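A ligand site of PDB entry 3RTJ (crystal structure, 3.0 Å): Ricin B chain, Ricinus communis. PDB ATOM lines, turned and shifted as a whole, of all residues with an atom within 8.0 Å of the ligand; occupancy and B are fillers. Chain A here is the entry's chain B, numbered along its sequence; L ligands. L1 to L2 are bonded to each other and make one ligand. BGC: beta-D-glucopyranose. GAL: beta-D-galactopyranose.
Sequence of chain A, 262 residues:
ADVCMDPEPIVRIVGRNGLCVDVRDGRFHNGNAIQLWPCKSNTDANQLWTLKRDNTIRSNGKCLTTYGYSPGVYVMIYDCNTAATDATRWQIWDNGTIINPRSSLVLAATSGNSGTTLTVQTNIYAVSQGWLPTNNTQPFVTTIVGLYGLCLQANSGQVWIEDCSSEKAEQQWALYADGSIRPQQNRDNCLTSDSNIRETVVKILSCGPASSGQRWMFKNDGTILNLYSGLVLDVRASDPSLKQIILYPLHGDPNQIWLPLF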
ATOM      1  N   CYS A  20      -3.212   7.731 -26.722  1.00  0.00           N
ATOM      2  CA  CYS A  20      -1.762   7.727 -26.493  1.00  0.00           C
ATOM      3  C   CYS A  20      -1.202   6.496 -25.799  1.00  0.00           C
ATOM      4  O   CYS A  20      -1.915   5.804 -25.073  1.00  0.00           O
ATOM      5  CB  CYS A  20      -1.381   8.972 -25.705  1.00  0.00           C
ATOM      6  SG  CYS A  20      -1.225  10.440 -26.777  1.00  0.00           S
ATOM      7  N   VAL A  21       0.082   6.208 -26.041  1.00  0.00           N
ATOM      8  CA  VAL A  21       0.744   5.076 -25.405  1.00  0.00           C
ATOM      9  C   VAL A  21       1.044   5.576 -24.004  1.00  0.00           C
ATOM     10  O   VAL A  21       1.886   6.453 -23.810  1.00  0.00           O
ATOM     11  CB  VAL A  21       2.039   4.673 -26.115  1.00  0.00           C
ATOM     12  CG1 VAL A  21       2.712   3.538 -25.348  1.00  0.00           C
ATOM     13  CG2 VAL A  21       1.737   4.229 -27.526  1.00  0.00           C
ATOM     14  N   ASP A  22       0.328   4.998 -23.054  1.00  0.00           N
ATOM     15  CA  ASP A  22       0.341   5.354 -21.637  1.00  0.00           C
ATOM     16  C   ASP A  22       0.869   4.235 -20.705  1.00  0.00           C
ATOM     17  O   ASP A  22       0.600   3.051 -20.932  1.00  0.00           O
ATOM     18  CB  ASP A  22      -1.127   5.697 -21.332  1.00  0.00           C
ATOM     19  CG  ASP A  22      -1.358   6.251 -19.965  1.00  0.00           C
ATOM     20  OD1 ASP A  22      -1.125   5.524 -18.971  1.00  0.00           O
ATOM     21  OD2 ASP A  22      -1.799   7.410 -19.873  1.00  0.00           O
ATOM     22  N   VAL A  23       1.635   4.593 -19.673  1.00  0.00           N
ATOM     23  CA  VAL A  23       2.120   3.587 -18.720  1.00  0.00           C
ATOM     24  C   VAL A  23       1.100   3.598 -17.585  1.00  0.00           C
ATOM     25  O   VAL A  23       1.026   4.570 -16.821  1.00  0.00           O
ATOM     26  CB  VAL A  23       3.495   3.957 -18.129  1.00  0.00           C
ATOM     27  CG1 VAL A  23       4.053   2.787 -17.310  1.00  0.00           C
ATOM     28  CG2 VAL A  23       4.449   4.318 -19.247  1.00  0.00           C
ATOM     29  N   ARG A  24       0.320   2.525 -17.482  1.00  0.00           N
ATOM     30  CA  ARG A  24      -0.764   2.400 -16.490  1.00  0.00           C
ATOM     31  C   ARG A  24      -0.532   2.932 -15.083  1.00  0.00           C
ATOM     32  O   ARG A  24       0.464   2.612 -14.431  1.00  0.00           O
ATOM     33  CB  ARG A  24      -1.223   0.949 -16.409  1.00  0.00           C
ATOM     34  CG  ARG A  24      -2.453   0.737 -15.528  1.00  0.00           C
ATOM     35  CD  ARG A  24      -3.038  -0.645 -15.723  1.00  0.00           C
ATOM     36  NE  ARG A  24      -3.729  -0.777 -17.002  1.00  0.00           N
ATOM     37  CZ  ARG A  24      -3.809  -1.895 -17.709  1.00  0.00           C
ATOM     38  NH1 ARG A  24      -3.223  -3.005 -17.266  1.00  0.00           N
ATOM     39  NH2 ARG A  24      -4.462  -1.913 -18.857  1.00  0.00           N
ATOM     40  N   ASP A  25      -1.491   3.736 -14.635  1.00  0.00           N
ATOM     41  CA  ASP A  25      -1.515   4.369 -13.305  1.00  0.00           C
ATOM     42  C   ASP A  25      -0.233   5.095 -12.875  1.00  0.00           C
ATOM     43  O   ASP A  25       0.012   5.264 -11.689  1.00  0.00           O
ATOM     44  CB  ASP A  25      -1.904   3.344 -12.242  1.00  0.00           C
ATOM     45  CG  ASP A  25      -3.286   2.759 -12.478  1.00  0.00           C
ATOM     46  OD1 ASP A  25      -4.212   3.543 -12.766  1.00  0.00           O
ATOM     47  OD2 ASP A  25      -3.439   1.515 -12.373  1.00  0.00           O
ATOM     48  N   GLY A  26       0.561   5.539 -13.841  1.00  0.00           N
ATOM     49  CA  GLY A  26       1.782   6.262 -13.513  1.00  0.00           C
ATOM     50  C   GLY A  26       2.848   5.504 -12.729  1.00  0.00           C
ATOM     51  O   GLY A  26       3.806   6.117 -12.268  1.00  0.00           O
ATOM     52  N   ARG A  27       2.698   4.194 -12.584  1.00  0.00           N
ATOM     53  CA  ARG A  27       3.686   3.416 -11.828  1.00  0.00           C
ATOM     54  C   ARG A  27       4.731   2.735 -12.727  1.00  0.00           C
ATOM     55  O   ARG A  27       4.414   2.321 -13.849  1.00  0.00           O
ATOM     56  CB  ARG A  27       2.988   2.348 -11.005  1.00  0.00           C
ATOM     57  CG  ARG A  27       1.702   2.808 -10.391  1.00  0.00           C
ATOM     58  CD  ARG A  27       1.377   1.919  -9.221  1.00  0.00           C
ATOM     59  NE  ARG A  27       2.045   2.364  -8.006  1.00  0.00           N
ATOM     60  CZ  ARG A  27       1.631   3.398  -7.286  1.00  0.00           C
ATOM     61  NH1 ARG A  27       0.561   4.085  -7.655  1.00  0.00           N
ATOM     62  NH2 ARG A  27       2.300   3.740  -6.189  1.00  0.00           N
ATOM     63  N   ASN A  32       4.459  -3.601 -14.950  1.00  0.00           N
ATOM     64  CA  ASN A  32       3.234  -2.805 -15.078  1.00  0.00           C
ATOM     65  C   ASN A  32       2.946  -2.666 -16.572  1.00  0.00           C
ATOM     66  O   ASN A  32       3.850  -2.409 -17.364  1.00  0.00           O
ATOM     67  CB  ASN A  32       3.412  -1.420 -14.423  1.00  0.00           C
ATOM     68  CG  ASN A  32       2.117  -0.630 -14.350  1.00  0.00           C
ATOM     69  OD1 ASN A  32       1.083  -1.154 -13.939  1.00  0.00           O
ATOM     70  ND2 ASN A  32       2.174   0.637 -14.742  1.00  0.00           N
ATOM     71  N   ALA A  33       1.690  -2.872 -16.958  1.00  0.00           N
ATOM     72  CA  ALA A  33       1.299  -2.827 -18.367  1.00  0.00           C
ATOM     73  C   ALA A  33       1.367  -1.471 -19.041  1.00  0.00           C
ATOM     74  O   ALA A  33       1.452  -0.431 -18.399  1.00  0.00           O
ATOM     75  CB  ALA A  33      -0.103  -3.411 -18.539  1.00  0.00           C
ATOM     76  N   GLN A  35      -0.710   0.808 -21.873  1.00  0.00           N
ATOM     77  CA  GLN A  35      -2.086   0.838 -22.364  1.00  0.00           C
ATOM     78  C   GLN A  35      -2.437   2.043 -23.226  1.00  0.00           C
ATOM     79  O   GLN A  35      -1.662   2.993 -23.313  1.00  0.00           O
ATOM     80  CB  GLN A  35      -3.029   0.827 -21.157  1.00  0.00           C
ATOM     81  CG  GLN A  35      -2.543   1.712 -20.021  1.00  0.00           C
ATOM     82  CD  GLN A  35      -3.641   2.103 -19.043  1.00  0.00           C
ATOM     83  OE1 GLN A  35      -4.474   1.292 -18.659  1.00  0.00           O
ATOM     84  NE2 GLN A  35      -3.631   3.358 -18.622  1.00  0.00           N
ATOM     85  N   LEU A  36      -3.599   1.977 -23.872  1.00  0.00           N
ATOM     86  CA  LEU A  36      -4.075   3.093 -24.679  1.00  0.00           C
ATOM     87  C   LEU A  36      -4.777   3.995 -23.679  1.00  0.00           C
ATOM     88  O   LEU A  36      -5.484   3.525 -22.791  1.00  0.00           O
ATOM     89  CB  LEU A  36      -5.096   2.630 -25.722  1.00  0.00           C
ATOM     90  CG  LEU A  36      -4.600   2.181 -27.091  1.00  0.00           C
ATOM     91  CD1 LEU A  36      -5.802   1.910 -27.967  1.00  0.00           C
ATOM     92  CD2 LEU A  36      -3.727   3.248 -27.721  1.00  0.00           C
ATOM     93  N   TRP A  37      -4.585   5.302 -23.807  1.00  0.00           N
ATOM     94  CA  TRP A  37      -5.195   6.204 -22.869  1.00  0.00           C
ATOM     95  C   TRP A  37      -5.288   7.598 -23.433  1.00  0.00           C
ATOM     96  O   TRP A  37      -4.364   8.061 -24.089  1.00  0.00           O
ATOM     97  CB  TRP A  37      -4.378   6.217 -21.579  1.00  0.00           C
ATOM     98  CG  TRP A  37      -5.098   6.813 -20.431  1.00  0.00           C
ATOM     99  CD1 TRP A  37      -4.924   8.063 -19.903  1.00  0.00           C
ATOM    100  CD2 TRP A  37      -6.156   6.205 -19.696  1.00  0.00           C
ATOM    101  NE1 TRP A  37      -5.798   8.261 -18.868  1.00  0.00           N
ATOM    102  CE2 TRP A  37      -6.569   7.141 -18.714  1.00  0.00           C
ATOM    103  CE3 TRP A  37      -6.787   4.950 -19.749  1.00  0.00           C
ATOM    104  CZ2 TRP A  37      -7.602   6.864 -17.807  1.00  0.00           C
ATOM    105  CZ3 TRP A  37      -7.810   4.675 -18.843  1.00  0.00           C
ATOM    106  CH2 TRP A  37      -8.207   5.632 -17.886  1.00  0.00           C
ATOM    107  N   PRO A  38      -6.410   8.294 -23.194  1.00  0.00           N
ATOM    108  CA  PRO A  38      -6.600   9.667 -23.685  1.00  0.00           C
ATOM    109  C   PRO A  38      -5.324  10.465 -23.448  1.00  0.00           C
ATOM    110  O   PRO A  38      -4.740  10.422 -22.357  1.00  0.00           O
ATOM    111  CB  PRO A  38      -7.770  10.156 -22.850  1.00  0.00           C
ATOM    112  CG  PRO A  38      -8.619   8.920 -22.763  1.00  0.00           C
ATOM    113  CD  PRO A  38      -7.601   7.843 -22.456  1.00  0.00           C
ATOM    114  N   CYS A  39      -4.882  11.186 -24.469  1.00  0.00           N
ATOM    115  CA  CYS A  39      -3.665  11.975 -24.376  1.00  0.00           C
ATOM    116  C   CYS A  39      -3.757  13.135 -23.409  1.00  0.00           C
ATOM    117  O   CYS A  39      -4.766  13.830 -23.332  1.00  0.00           O
ATOM    118  CB  CYS A  39      -3.258  12.460 -25.758  1.00  0.00           C
ATOM    119  SG  CYS A  39      -3.116  11.147 -27.005  1.00  0.00           S
ATOM    120  N   LYS A  40      -2.657  13.357 -22.686  1.00  0.00           N
ATOM    121  CA  LYS A  40      -2.604  14.410 -21.702  1.00  0.00           C
ATOM    122  C   LYS A  40      -1.882  15.664 -22.149  1.00  0.00           C
ATOM    123  O   LYS A  40      -0.942  15.597 -22.946  1.00  0.00           O
ATOM    124  CB  LYS A  40      -1.948  13.867 -20.425  1.00  0.00           C
ATOM    125  CG  LYS A  40      -2.719  12.703 -19.838  1.00  0.00           C
ATOM    126  CD  LYS A  40      -2.257  12.362 -18.445  1.00  0.00           C
ATOM    127  CE  LYS A  40      -0.874  11.738 -18.430  1.00  0.00           C
ATOM    128  NZ  LYS A  40      -0.639  11.111 -17.101  1.00  0.00           N
ATOM    129  N   ASN A  42       0.270  17.941 -20.574  1.00  0.00           N
ATOM    130  CA  ASN A  42       1.135  18.221 -19.438  1.00  0.00           C
ATOM    131  C   ASN A  42       2.484  17.514 -19.595  1.00  0.00           C
ATOM    132  O   ASN A  42       2.894  17.186 -20.701  1.00  0.00           O
ATOM    133  CB  ASN A  42       0.474  17.779 -18.137  1.00  0.00           C
ATOM    134  CG  ASN A  42      -0.053  16.365 -18.216  1.00  0.00           C
ATOM    135  OD1 ASN A  42       0.703  15.409 -18.384  1.00  0.00           O
ATOM    136  ND2 ASN A  42      -1.373  16.229 -18.121  1.00  0.00           N
ATOM    137  N   ASP A  44       3.408  14.624 -17.547  1.00  0.00           N
ATOM    138  CA  ASP A  44       3.441  13.323 -16.887  1.00  0.00           C
ATOM    139  C   ASP A  44       4.273  12.335 -17.709  1.00  0.00           C
ATOM    140  O   ASP A  44       3.846  11.865 -18.767  1.00  0.00           O
ATOM    141  CB  ASP A  44       2.020  12.786 -16.673  1.00  0.00           C
ATOM    142  CG  ASP A  44       1.189  13.717 -15.805  1.00  0.00           C
ATOM    143  OD1 ASP A  44       1.767  14.350 -14.901  1.00  0.00           O
ATOM    144  OD2 ASP A  44      -0.054  13.803 -16.021  1.00  0.00           O
ATOM    145  N   ALA A  45       5.478  12.043 -17.213  1.00  0.00           N
ATOM    146  CA  ALA A  45       6.424  11.149 -17.889  1.00  0.00           C
ATOM    147  C   ALA A  45       5.875   9.786 -18.259  1.00  0.00           C
ATOM    148  O   ALA A  45       6.546   9.040 -18.979  1.00  0.00           O
ATOM    149  CB  ALA A  45       7.676  10.981 -17.026  1.00  0.00           C
ATOM    150  N   ASN A  46       4.678   9.457 -17.802  1.00  0.00           N
ATOM    151  CA  ASN A  46       4.095   8.163 -18.120  1.00  0.00           C
ATOM    152  C   ASN A  46       3.448   8.160 -19.500  1.00  0.00           C
ATOM    153  O   ASN A  46       2.865   7.162 -19.922  1.00  0.00           O
ATOM    154  CB  ASN A  46       3.082   7.737 -17.049  1.00  0.00           C
ATOM    155  CG  ASN A  46       1.689   8.258 -17.327  1.00  0.00           C
ATOM    156  OD1 ASN A  46       1.498   9.438 -17.597  1.00  0.00           O
ATOM    157  ND2 ASN A  46       0.696   7.374 -17.237  1.00  0.00           N
ATOM    158  N   GLN A  47       3.541   9.289 -20.197  1.00  0.00           N
ATOM    159  CA  GLN A  47       2.956   9.389 -21.529  1.00  0.00           C
ATOM    160  C   GLN A  47       3.920   9.949 -22.574  1.00  0.00           C
ATOM    161  O   GLN A  47       3.573  10.030 -23.758  1.00  0.00           O
ATOM    162  CB  GLN A  47       1.674  10.216 -21.469  1.00  0.00           C
ATOM    163  CG  GLN A  47       0.497   9.522 -22.125  1.00  0.00           C
ATOM    164  CD  GLN A  47      -0.801  10.235 -21.909  1.00  0.00           C
ATOM    165  OE1 GLN A  47      -0.949  11.400 -22.268  1.00  0.00           O
ATOM    166  NE2 GLN A  47      -1.761   9.546 -21.328  1.00  0.00           N
ATOM    167  N   SER A 114     -10.448   2.921 -24.224  1.00  0.00           N
ATOM    168  CA  SER A 114      -9.483   3.557 -23.371  1.00  0.00           C
ATOM    169  C   SER A 114      -9.105   2.572 -22.267  1.00  0.00           C
ATOM    170  O   SER A 114      -9.996   1.995 -21.633  1.00  0.00           O
ATOM    171  CB  SER A 114     -10.088   4.823 -22.771  1.00  0.00           C
ATOM    172  OG  SER A 114      -9.154   5.461 -21.913  1.00  0.00           O
ATOM    173  N   GLY A 115      -7.819   2.376 -22.059  1.00  0.00           N
ATOM    174  CA  GLY A 115      -7.363   1.461 -21.016  1.00  0.00           C
ATOM    175  C   GLY A 115      -6.914   0.106 -21.533  1.00  0.00           C
ATOM    176  O   GLY A 115      -6.391  -0.694 -20.774  1.00  0.00           O
HETATM  177  C2  BGC L   1      -4.591   6.587  -9.733  1.00  0.00           C
HETATM  178  C3  BGC L   1      -4.105   6.532 -11.187  1.00  0.00           C
HETATM  179  C4  BGC L   1      -3.685   7.918 -11.732  1.00  0.00           C
HETATM  180  C5  BGC L   1      -2.870   8.739 -10.710  1.00  0.00           C
HETATM  181  C6  BGC L   1      -2.762  10.197 -11.113  1.00  0.00           C
HETATM  182  C1  BGC L   1      -3.574   7.365  -8.890  1.00  0.00           C
HETATM  183  O1  BGC L   1      -3.982   7.433  -7.571  1.00  0.00           O
HETATM  184  O2  BGC L   1      -4.738   5.269  -9.205  1.00  0.00           O
HETATM  185  O3  BGC L   1      -5.142   6.005 -12.005  1.00  0.00           O
HETATM  186  O4  BGC L   1      -2.876   7.737 -12.916  1.00  0.00           O
HETATM  187  O5  BGC L   1      -3.481   8.697  -9.400  1.00  0.00           O
HETATM  188  O6  BGC L   1      -4.009  10.700 -11.569  1.00  0.00           O
HETATM  189  C1  GAL L   2      -3.465   7.852 -14.165  1.00  0.00           C
HETATM  190  C2  GAL L   2      -2.370   8.223 -15.186  1.00  0.00           C
HETATM  191  C3  GAL L   2      -2.915   8.174 -16.612  1.00  0.00           C
HETATM  192  C4  GAL L   2      -3.556   6.810 -16.884  1.00  0.00           C
HETATM  193  C5  GAL L   2      -4.630   6.539 -15.822  1.00  0.00           C
HETATM  194  C6  GAL L   2      -5.324   5.186 -15.982  1.00  0.00           C
HETATM  195  O2  GAL L   2      -1.869   9.521 -14.915  1.00  0.00           O
HETATM  196  O3  GAL L   2      -1.855   8.417 -17.533  1.00  0.00           O
HETATM  197  O4  GAL L   2      -2.560   5.784 -16.831  1.00  0.00           O
HETATM  198  O5  GAL L   2      -4.052   6.577 -14.494  1.00  0.00           O
HETATM  199  O6  GAL L   2      -4.399   4.108 -15.929  1.00  0.00           O
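An oxygen (O3) of BGC L1 sits at hydrogen-bond distance from the side-chain carboxylate (OD1) of Asp 25 (2.7 Å). NZ of Lys 40 is in hydrogen-bond range of O2 of GAL L2. The side-chain amide nitrogen (NE2) of Gln 35 lies within hydrogen-bond range of an oxygen (O6) of GAL L2 (2.9 Å). An oxygen (O3) of GAL L2 is in hydrogen-bond range of the side-chain amide nitrogen of Asn 46 (2.8 Å). The side-chain carboxylate of Asp 22 is in hydrogen-bond range of an oxygen (O3) of GAL L2 (2.5 Å). The backbone NH (N) of Asp 25 lies within hydrogen-bond range of an oxygen (O4) of GAL L2 (3.2 Å).
The guanidinium group (NH2) of Arg 24 is in hydrogen-bond range of the backbone carbonyl oxygen (O) of Gly 115 (3.0 Å). The side-chain carboxylate (OD2) of Asp 22 lies within hydrogen-bond range of the side-chain amide nitrogen (NE2) of Gln 47. O of Asp 22 lies within hydrogen-bond range of N of Gln 35, 2.8 Å away. The side-chain amide nitrogen of Asn 32 is in hydrogen-bond range of the backbone carbonyl oxygen of Arg 24. The side-chain amide nitrogen (ND2) of Asn 46 lies within hydrogen-bond range of the backbone carbonyl oxygen (O) of Val 23 (2.9 Å). O of Ala 33 sits at hydrogen-bond distance from N of Arg 24, 3.3 Å away. The side-chain amide oxygen of Gln 35 sits at hydrogen-bond distance from the guanidinium group of Arg 24, at 2.8 Å. NZ of Lys 40 is in salt-bridge range of OD2 of Asp 44, at 3.0 Å.
O of Val 23 touches O4 of GAL L2, 3.8 Å away. CA of Arg 24 touches O4 of GAL L2 (3.8 Å). NE1 of Trp 37 touches C4 of GAL L2 (3.3 Å). NE2 of Gln 47 touches O3 of GAL L2, 3.96 Å away.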
